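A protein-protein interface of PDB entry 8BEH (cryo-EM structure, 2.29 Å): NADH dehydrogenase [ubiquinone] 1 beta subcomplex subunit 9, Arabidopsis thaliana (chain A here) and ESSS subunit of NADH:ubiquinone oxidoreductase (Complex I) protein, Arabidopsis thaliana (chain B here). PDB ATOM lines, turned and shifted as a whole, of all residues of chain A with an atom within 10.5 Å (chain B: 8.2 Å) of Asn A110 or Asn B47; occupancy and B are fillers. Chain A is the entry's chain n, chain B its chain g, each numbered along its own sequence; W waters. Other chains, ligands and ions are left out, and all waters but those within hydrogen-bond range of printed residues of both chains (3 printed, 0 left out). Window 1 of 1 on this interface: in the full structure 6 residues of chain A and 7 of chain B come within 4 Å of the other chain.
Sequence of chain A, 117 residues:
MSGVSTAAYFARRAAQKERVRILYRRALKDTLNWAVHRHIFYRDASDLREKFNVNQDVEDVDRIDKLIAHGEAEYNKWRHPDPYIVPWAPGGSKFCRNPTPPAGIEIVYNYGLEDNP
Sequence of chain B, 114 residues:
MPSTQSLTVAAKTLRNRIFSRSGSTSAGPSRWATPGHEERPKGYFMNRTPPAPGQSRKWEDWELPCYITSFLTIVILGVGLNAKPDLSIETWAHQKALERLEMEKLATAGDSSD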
ATOM      1  N   GLU A 106     -24.874  -8.339  -2.510  1.00  0.00           N
ATOM      2  CA  GLU A 106     -25.316  -7.333  -1.522  1.00  0.00           C
ATOM      3  C   GLU A 106     -24.610  -5.981  -1.761  1.00  0.00           C
ATOM      4  O   GLU A 106     -23.428  -5.993  -2.048  1.00  0.00           O
ATOM      5  CB  GLU A 106     -25.094  -7.926  -0.139  1.00  0.00           C
ATOM      6  CG  GLU A 106     -25.826  -9.222   0.073  1.00  0.00           C
ATOM      7  CD  GLU A 106     -25.221 -10.147   1.105  1.00  0.00           C
ATOM      8  OE1 GLU A 106     -24.872  -9.667   2.182  1.00  0.00           O
ATOM      9  OE2 GLU A 106     -25.125 -11.361   0.825  1.00  0.00           O
ATOM     10  N   ILE A 107     -25.305  -4.874  -1.684  1.00  0.00           N
ATOM     11  CA  ILE A 107     -24.722  -3.546  -1.820  1.00  0.00           C
ATOM     12  C   ILE A 107     -24.735  -2.895  -0.447  1.00  0.00           C
ATOM     13  O   ILE A 107     -25.779  -2.858   0.215  1.00  0.00           O
ATOM     14  CB  ILE A 107     -25.501  -2.696  -2.841  1.00  0.00           C
ATOM     15  CG1 ILE A 107     -25.487  -3.347  -4.230  1.00  0.00           C
ATOM     16  CG2 ILE A 107     -24.940  -1.290  -2.906  1.00  0.00           C
ATOM     17  CD1 ILE A 107     -24.121  -3.675  -4.770  1.00  0.00           C
ATOM     18  N   VAL A 108     -23.615  -2.388   0.003  1.00  0.00           N
ATOM     19  CA  VAL A 108     -23.507  -1.818   1.381  1.00  0.00           C
ATOM     20  C   VAL A 108     -23.578  -0.303   1.281  1.00  0.00           C
ATOM     21  O   VAL A 108     -22.977   0.296   0.388  1.00  0.00           O
ATOM     22  CB  VAL A 108     -22.230  -2.253   2.153  1.00  0.00           C
ATOM     23  CG1 VAL A 108     -22.146  -1.782   3.584  1.00  0.00           C
ATOM     24  CG2 VAL A 108     -21.862  -3.702   1.989  1.00  0.00           C
ATOM     25  N   TYR A 109     -24.252   0.273   2.214  1.00  0.00           N
ATOM     26  CA  TYR A 109     -24.430   1.708   2.343  1.00  0.00           C
ATOM     27  C   TYR A 109     -23.658   2.210   3.555  1.00  0.00           C
ATOM     28  O   TYR A 109     -23.385   1.453   4.490  1.00  0.00           O
ATOM     29  CB  TYR A 109     -25.914   2.058   2.482  1.00  0.00           C
ATOM     30  CG  TYR A 109     -26.701   1.891   1.208  1.00  0.00           C
ATOM     31  CD1 TYR A 109     -26.089   2.009  -0.033  1.00  0.00           C
ATOM     32  CD2 TYR A 109     -28.048   1.567   1.245  1.00  0.00           C
ATOM     33  CE1 TYR A 109     -26.809   1.847  -1.198  1.00  0.00           C
ATOM     34  CE2 TYR A 109     -28.772   1.399   0.092  1.00  0.00           C
ATOM     35  CZ  TYR A 109     -28.150   1.538  -1.128  1.00  0.00           C
ATOM     36  OH  TYR A 109     -28.877   1.370  -2.278  1.00  0.00           O
ATOM     37  N   ASN A 110     -23.292   3.493   3.517  1.00  0.00           N
ATOM     38  CA  ASN A 110     -22.646   4.180   4.637  1.00  0.00           C
ATOM     39  C   ASN A 110     -21.327   3.514   5.032  1.00  0.00           C
ATOM     40  O   ASN A 110     -21.025   3.321   6.209  1.00  0.00           O
ATOM     41  CB  ASN A 110     -23.596   4.275   5.836  1.00  0.00           C
ATOM     42  CG  ASN A 110     -24.981   4.740   5.441  1.00  0.00           C
ATOM     43  OD1 ASN A 110     -25.141   5.783   4.813  1.00  0.00           O
ATOM     44  ND2 ASN A 110     -25.988   3.963   5.798  1.00  0.00           N
ATOM     45  N   TYR A 111     -20.531   3.174   4.027  1.00  0.00           N
ATOM     46  CA  TYR A 111     -19.206   2.618   4.238  1.00  0.00           C
ATOM     47  C   TYR A 111     -18.182   3.725   4.470  1.00  0.00           C
ATOM     48  O   TYR A 111     -18.313   4.840   3.961  1.00  0.00           O
ATOM     49  CB  TYR A 111     -18.787   1.766   3.039  1.00  0.00           C
ATOM     50  CG  TYR A 111     -17.437   1.109   3.193  1.00  0.00           C
ATOM     51  CD1 TYR A 111     -17.272  -0.005   4.006  1.00  0.00           C
ATOM     52  CD2 TYR A 111     -16.323   1.610   2.534  1.00  0.00           C
ATOM     53  CE1 TYR A 111     -16.041  -0.603   4.152  1.00  0.00           C
ATOM     54  CE2 TYR A 111     -15.089   1.021   2.675  1.00  0.00           C
ATOM     55  CZ  TYR A 111     -14.953  -0.089   3.488  1.00  0.00           C
ATOM     56  OH  TYR A 111     -13.723  -0.683   3.634  1.00  0.00           O
ATOM     57  N   GLY A 112     -17.160   3.403   5.257  1.00  0.00           N
ATOM     58  CA  GLY A 112     -16.031   4.292   5.451  1.00  0.00           C
ATOM     59  C   GLY A 112     -16.322   5.593   6.169  1.00  0.00           C
ATOM     60  O   GLY A 112     -15.679   6.602   5.879  1.00  0.00           O
ATOM     61  N   LEU A 113     -17.267   5.594   7.103  1.00  0.00           N
ATOM     62  CA  LEU A 113     -17.569   6.794   7.868  1.00  0.00           C
ATOM     63  C   LEU A 113     -16.444   7.101   8.852  1.00  0.00           C
ATOM     64  O   LEU A 113     -15.709   6.211   9.284  1.00  0.00           O
ATOM     65  CB  LEU A 113     -18.893   6.627   8.611  1.00  0.00           C
ATOM     66  CG  LEU A 113     -20.091   6.367   7.694  1.00  0.00           C
ATOM     67  CD1 LEU A 113     -21.320   5.957   8.479  1.00  0.00           C
ATOM     68  CD2 LEU A 113     -20.374   7.598   6.860  1.00  0.00           C
ATOM     69  N   GLU A 114     -16.305   8.382   9.195  1.00  0.00           N
ATOM     70  CA  GLU A 114     -15.223   8.781  10.089  1.00  0.00           C
ATOM     71  C   GLU A 114     -15.384   8.182  11.479  1.00  0.00           C
ATOM     72  O   GLU A 114     -14.390   7.981  12.183  1.00  0.00           O
ATOM     73  CB  GLU A 114     -15.127  10.305  10.169  1.00  0.00           C
ATOM     74  CG  GLU A 114     -16.438  11.025  10.384  1.00  0.00           C
ATOM     75  CD  GLU A 114     -16.237  12.489  10.736  1.00  0.00           C
ATOM     76  OE1 GLU A 114     -15.175  13.037  10.394  1.00  0.00           O
ATOM     77  OE2 GLU A 114     -17.146  13.099  11.333  1.00  0.00           O
ATOM     78  N   ASP A 115     -16.612   7.891  11.893  1.00  0.00           N
ATOM     79  CA  ASP A 115     -16.849   7.302  13.202  1.00  0.00           C
ATOM     80  C   ASP A 115     -16.639   5.791  13.178  1.00  0.00           C
ATOM     81  O   ASP A 115     -16.569   5.148  14.225  1.00  0.00           O
ATOM     82  CB  ASP A 115     -18.260   7.627  13.690  1.00  0.00           C
ATOM     83  CG  ASP A 115     -18.422   9.084  14.070  1.00  0.00           C
ATOM     84  OD1 ASP A 115     -17.393   9.774  14.229  1.00  0.00           O
ATOM     85  OD2 ASP A 115     -19.575   9.541  14.208  1.00  0.00           O
ATOM     86  N   GLY B  43     -30.440   3.356  -6.234  1.00  0.00           N
ATOM     87  CA  GLY B  43     -29.230   3.664  -5.504  1.00  0.00           C
ATOM     88  C   GLY B  43     -29.310   4.982  -4.755  1.00  0.00           C
ATOM     89  O   GLY B  43     -30.301   5.709  -4.788  1.00  0.00           O
ATOM     90  N   TYR B  44     -28.222   5.289  -4.061  1.00  0.00           N
ATOM     91  CA  TYR B  44     -28.065   6.562  -3.376  1.00  0.00           C
ATOM     92  C   TYR B  44     -26.735   7.153  -3.793  1.00  0.00           C
ATOM     93  O   TYR B  44     -25.729   6.440  -3.838  1.00  0.00           O
ATOM     94  CB  TYR B  44     -28.124   6.391  -1.858  1.00  0.00           C
ATOM     95  CG  TYR B  44     -29.521   6.134  -1.368  1.00  0.00           C
ATOM     96  CD1 TYR B  44     -30.535   7.041  -1.617  1.00  0.00           C
ATOM     97  CD2 TYR B  44     -29.832   4.968  -0.684  1.00  0.00           C
ATOM     98  CE1 TYR B  44     -31.815   6.804  -1.194  1.00  0.00           C
ATOM     99  CE2 TYR B  44     -31.116   4.725  -0.249  1.00  0.00           C
ATOM    100  CZ  TYR B  44     -32.103   5.648  -0.506  1.00  0.00           C
ATOM    101  OH  TYR B  44     -33.388   5.418  -0.076  1.00  0.00           O
ATOM    102  N   PHE B  45     -26.732   8.443  -4.106  1.00  0.00           N
ATOM    103  CA  PHE B  45     -25.507   9.096  -4.535  1.00  0.00           C
ATOM    104  C   PHE B  45     -24.437   8.979  -3.458  1.00  0.00           C
ATOM    105  O   PHE B  45     -24.644   9.405  -2.317  1.00  0.00           O
ATOM    106  CB  PHE B  45     -25.774  10.558  -4.868  1.00  0.00           C
ATOM    107  CG  PHE B  45     -24.556  11.292  -5.327  1.00  0.00           C
ATOM    108  CD1 PHE B  45     -24.135  12.440  -4.681  1.00  0.00           C
ATOM    109  CD2 PHE B  45     -23.809  10.808  -6.384  1.00  0.00           C
ATOM    110  CE1 PHE B  45     -23.005  13.105  -5.099  1.00  0.00           C
ATOM    111  CE2 PHE B  45     -22.674  11.470  -6.806  1.00  0.00           C
ATOM    112  CZ  PHE B  45     -22.271  12.620  -6.162  1.00  0.00           C
ATOM    113  N   MET B  46     -23.297   8.399  -3.827  1.00  0.00           N
ATOM    114  CA  MET B  46     -22.185   8.128  -2.917  1.00  0.00           C
ATOM    115  C   MET B  46     -22.575   7.192  -1.773  1.00  0.00           C
ATOM    116  O   MET B  46     -21.952   7.215  -0.710  1.00  0.00           O
ATOM    117  CB  MET B  46     -21.573   9.437  -2.396  1.00  0.00           C
ATOM    118  CG  MET B  46     -20.926  10.241  -3.526  1.00  0.00           C
ATOM    119  SD  MET B  46     -20.449  11.946  -3.192  1.00  0.00           S
ATOM    120  CE  MET B  46     -21.383  12.288  -1.717  1.00  0.00           C
ATOM    121  N   ASN B  47     -23.599   6.364  -1.999  1.00  0.00           N
ATOM    122  CA  ASN B  47     -23.963   5.244  -1.122  1.00  0.00           C
ATOM    123  C   ASN B  47     -24.220   5.677   0.318  1.00  0.00           C
ATOM    124  O   ASN B  47     -23.951   4.936   1.263  1.00  0.00           O
ATOM    125  CB  ASN B  47     -22.900   4.139  -1.160  1.00  0.00           C
ATOM    126  CG  ASN B  47     -22.954   3.308  -2.429  1.00  0.00           C
ATOM    127  OD1 ASN B  47     -22.986   3.850  -3.531  1.00  0.00           O
ATOM    128  ND2 ASN B  47     -22.981   1.989  -2.279  1.00  0.00           N
ATOM    129  N   ARG B  48     -24.760   6.876   0.497  1.00  0.00           N
ATOM    130  CA  ARG B  48     -25.167   7.341   1.817  1.00  0.00           C
ATOM    131  C   ARG B  48     -26.686   7.341   1.896  1.00  0.00           C
ATOM    132  O   ARG B  48     -27.359   7.876   1.014  1.00  0.00           O
ATOM    133  CB  ARG B  48     -24.616   8.732   2.138  1.00  0.00           C
ATOM    134  CG  ARG B  48     -24.795   9.771   1.055  1.00  0.00           C
ATOM    135  CD  ARG B  48     -24.567  11.168   1.605  1.00  0.00           C
ATOM    136  NE  ARG B  48     -23.155  11.504   1.754  1.00  0.00           N
ATOM    137  CZ  ARG B  48     -22.610  12.636   1.336  1.00  0.00           C
ATOM    138  NH1 ARG B  48     -23.323  13.557   0.708  1.00  0.00           N
ATOM    139  NH2 ARG B  48     -21.313  12.843   1.536  1.00  0.00           N
ATOM    140  N   THR B  49     -27.220   6.726   2.940  1.00  0.00           N
ATOM    141  CA  THR B  49     -28.655   6.706   3.119  1.00  0.00           C
ATOM    142  C   THR B  49     -29.156   8.113   3.446  1.00  0.00           C
ATOM    143  O   THR B  49     -28.460   8.891   4.097  1.00  0.00           O
ATOM    144  CB  THR B  49     -29.049   5.730   4.217  1.00  0.00           C
ATOM    145  OG1 THR B  49     -28.386   6.086   5.436  1.00  0.00           O
ATOM    146  CG2 THR B  49     -28.648   4.324   3.825  1.00  0.00           C
ATOM    147  N   PRO B  50     -30.350   8.472   2.972  1.00  0.00           N
ATOM    148  CA  PRO B  50     -30.845   9.833   3.191  1.00  0.00           C
ATOM    149  C   PRO B  50     -31.120  10.087   4.661  1.00  0.00           C
ATOM    150  O   PRO B  50     -31.337   9.144   5.440  1.00  0.00           O
ATOM    151  CB  PRO B  50     -32.134   9.839   2.359  1.00  0.00           C
ATOM    152  CG  PRO B  50     -32.408   8.360   2.688  1.00  0.00           C
ATOM    153  CD  PRO B  50     -31.294   7.863   1.994  1.00  0.00           C
ATOM    154  N   PRO B  51     -31.079  11.339   5.096  1.00  0.00           N
ATOM    155  CA  PRO B  51     -31.421  11.644   6.488  1.00  0.00           C
ATOM    156  C   PRO B  51     -32.911  11.455   6.728  1.00  0.00           C
ATOM    157  O   PRO B  51     -33.719  11.378   5.801  1.00  0.00           O
ATOM    158  CB  PRO B  51     -30.990  13.101   6.651  1.00  0.00           C
ATOM    159  CG  PRO B  51     -31.046  13.659   5.277  1.00  0.00           C
ATOM    160  CD  PRO B  51     -30.709  12.545   4.338  1.00  0.00           C
ATOM    161  N   GLU B  60     -19.346  15.458   7.845  1.00  0.00           N
ATOM    162  CA  GLU B  60     -18.159  14.919   8.490  1.00  0.00           C
ATOM    163  C   GLU B  60     -17.137  16.026   8.733  1.00  0.00           C
ATOM    164  O   GLU B  60     -17.168  17.090   8.110  1.00  0.00           O
ATOM    165  CB  GLU B  60     -17.554  13.792   7.659  1.00  0.00           C
ATOM    166  CG  GLU B  60     -18.528  12.679   7.332  1.00  0.00           C
ATOM    167  CD  GLU B  60     -17.845  11.339   7.128  1.00  0.00           C
ATOM    168  OE1 GLU B  60     -16.932  11.259   6.281  1.00  0.00           O
ATOM    169  OE2 GLU B  60     -18.226  10.363   7.807  1.00  0.00           O
HETATM  170  O   HOH W   1     -15.231   9.290   5.842  1.00  0.00           O
HETATM  171  O   HOH W   2     -31.185   2.547  -3.263  1.00  0.00           O
HETATM  172  O   HOH W   3     -20.637   5.465   1.993  1.00  0.00           O
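N of Asn A110 lies within hydrogen-bond range of O of Asn B47 (2.8 Å). The side-chain carboxylate of Glu B60 lies within hydrogen-bond range of the backbone NH of Glu A114, 3.1 Å away. The backbone NH (N) of Thr B49 is in hydrogen-bond range of the side-chain amide oxygen (OD1) of Asn A110 (3.0 Å). The side-chain amide nitrogen of Asn B47 is in hydrogen-bond range of the backbone carbonyl oxygen of Val A108, 3.2 Å away.
Among the printed residues, merely in contact across the chains: Asn A110 with Arg B48, Tyr A109 with Asn B47, Leu A113 with Glu B60, Tyr A109 with Thr B49, Tyr A109 with Tyr B44, Ile A107 with Asn B47 and Tyr A109 with Gly B43.
Water W1 lies within hydrogen-bond range of OE1 of Glu B60 (2.6 Å) and O of Gly A112 (2.7 Å). Water W2 bridges OH of Tyr A109 (2.8 Å) and N of Gly B43 (3.2 Å). Water W3 lies within hydrogen-bond range of the backbone NH (N) of Tyr A111 (3.1 Å), the backbone carbonyl oxygen (O) of Asn B47 (3.4 Å) and the backbone carbonyl oxygen (O) of Met B46 (3.5 Å).
Of the printed residues of chain B, Tyr A109 touches Gly B43, Tyr B44, Asn B47 and Thr B49. Of the printed residues of chain B, Asn A110 touches Asn B47 (2.8 Å), Arg B48 (3.4 Å) and Thr B49 (3.0 Å). Gly A112 touches none of the printed residues of chain B. Of the printed residues of chain B, Glu A114 touches Glu B60. Of the printed residues of chain A, Gly B43 touches Tyr A109 (3.97 Å). Of chain A, only Ile A107, Val A108, Tyr A109 and Asn A110 come within 4 Å of Asn B47. Of the printed residues of chain A, Arg B48 touches Asn A110 (3.4 Å).
Hydrophobic or aromatic side chains of chain B within 4 Å of the printed part of chain A: Tyr B44. Along chain B the printed residues that touch a printed residue of chain A span positions 43 to 60. Hydrophobic or aromatic side chains of chain A that line the printed part of chain B: Ile A107, Tyr A109 and Leu A113. Along chain A the printed residues that touch a printed residue of chain B span positions 107 to 114. Among the printed residues, 11 pairs touch across the chains. Among the printed residues, no Asp or Glu carboxylate lies within 4 Å of a Lys or Arg side-chain nitrogen of the other chain.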
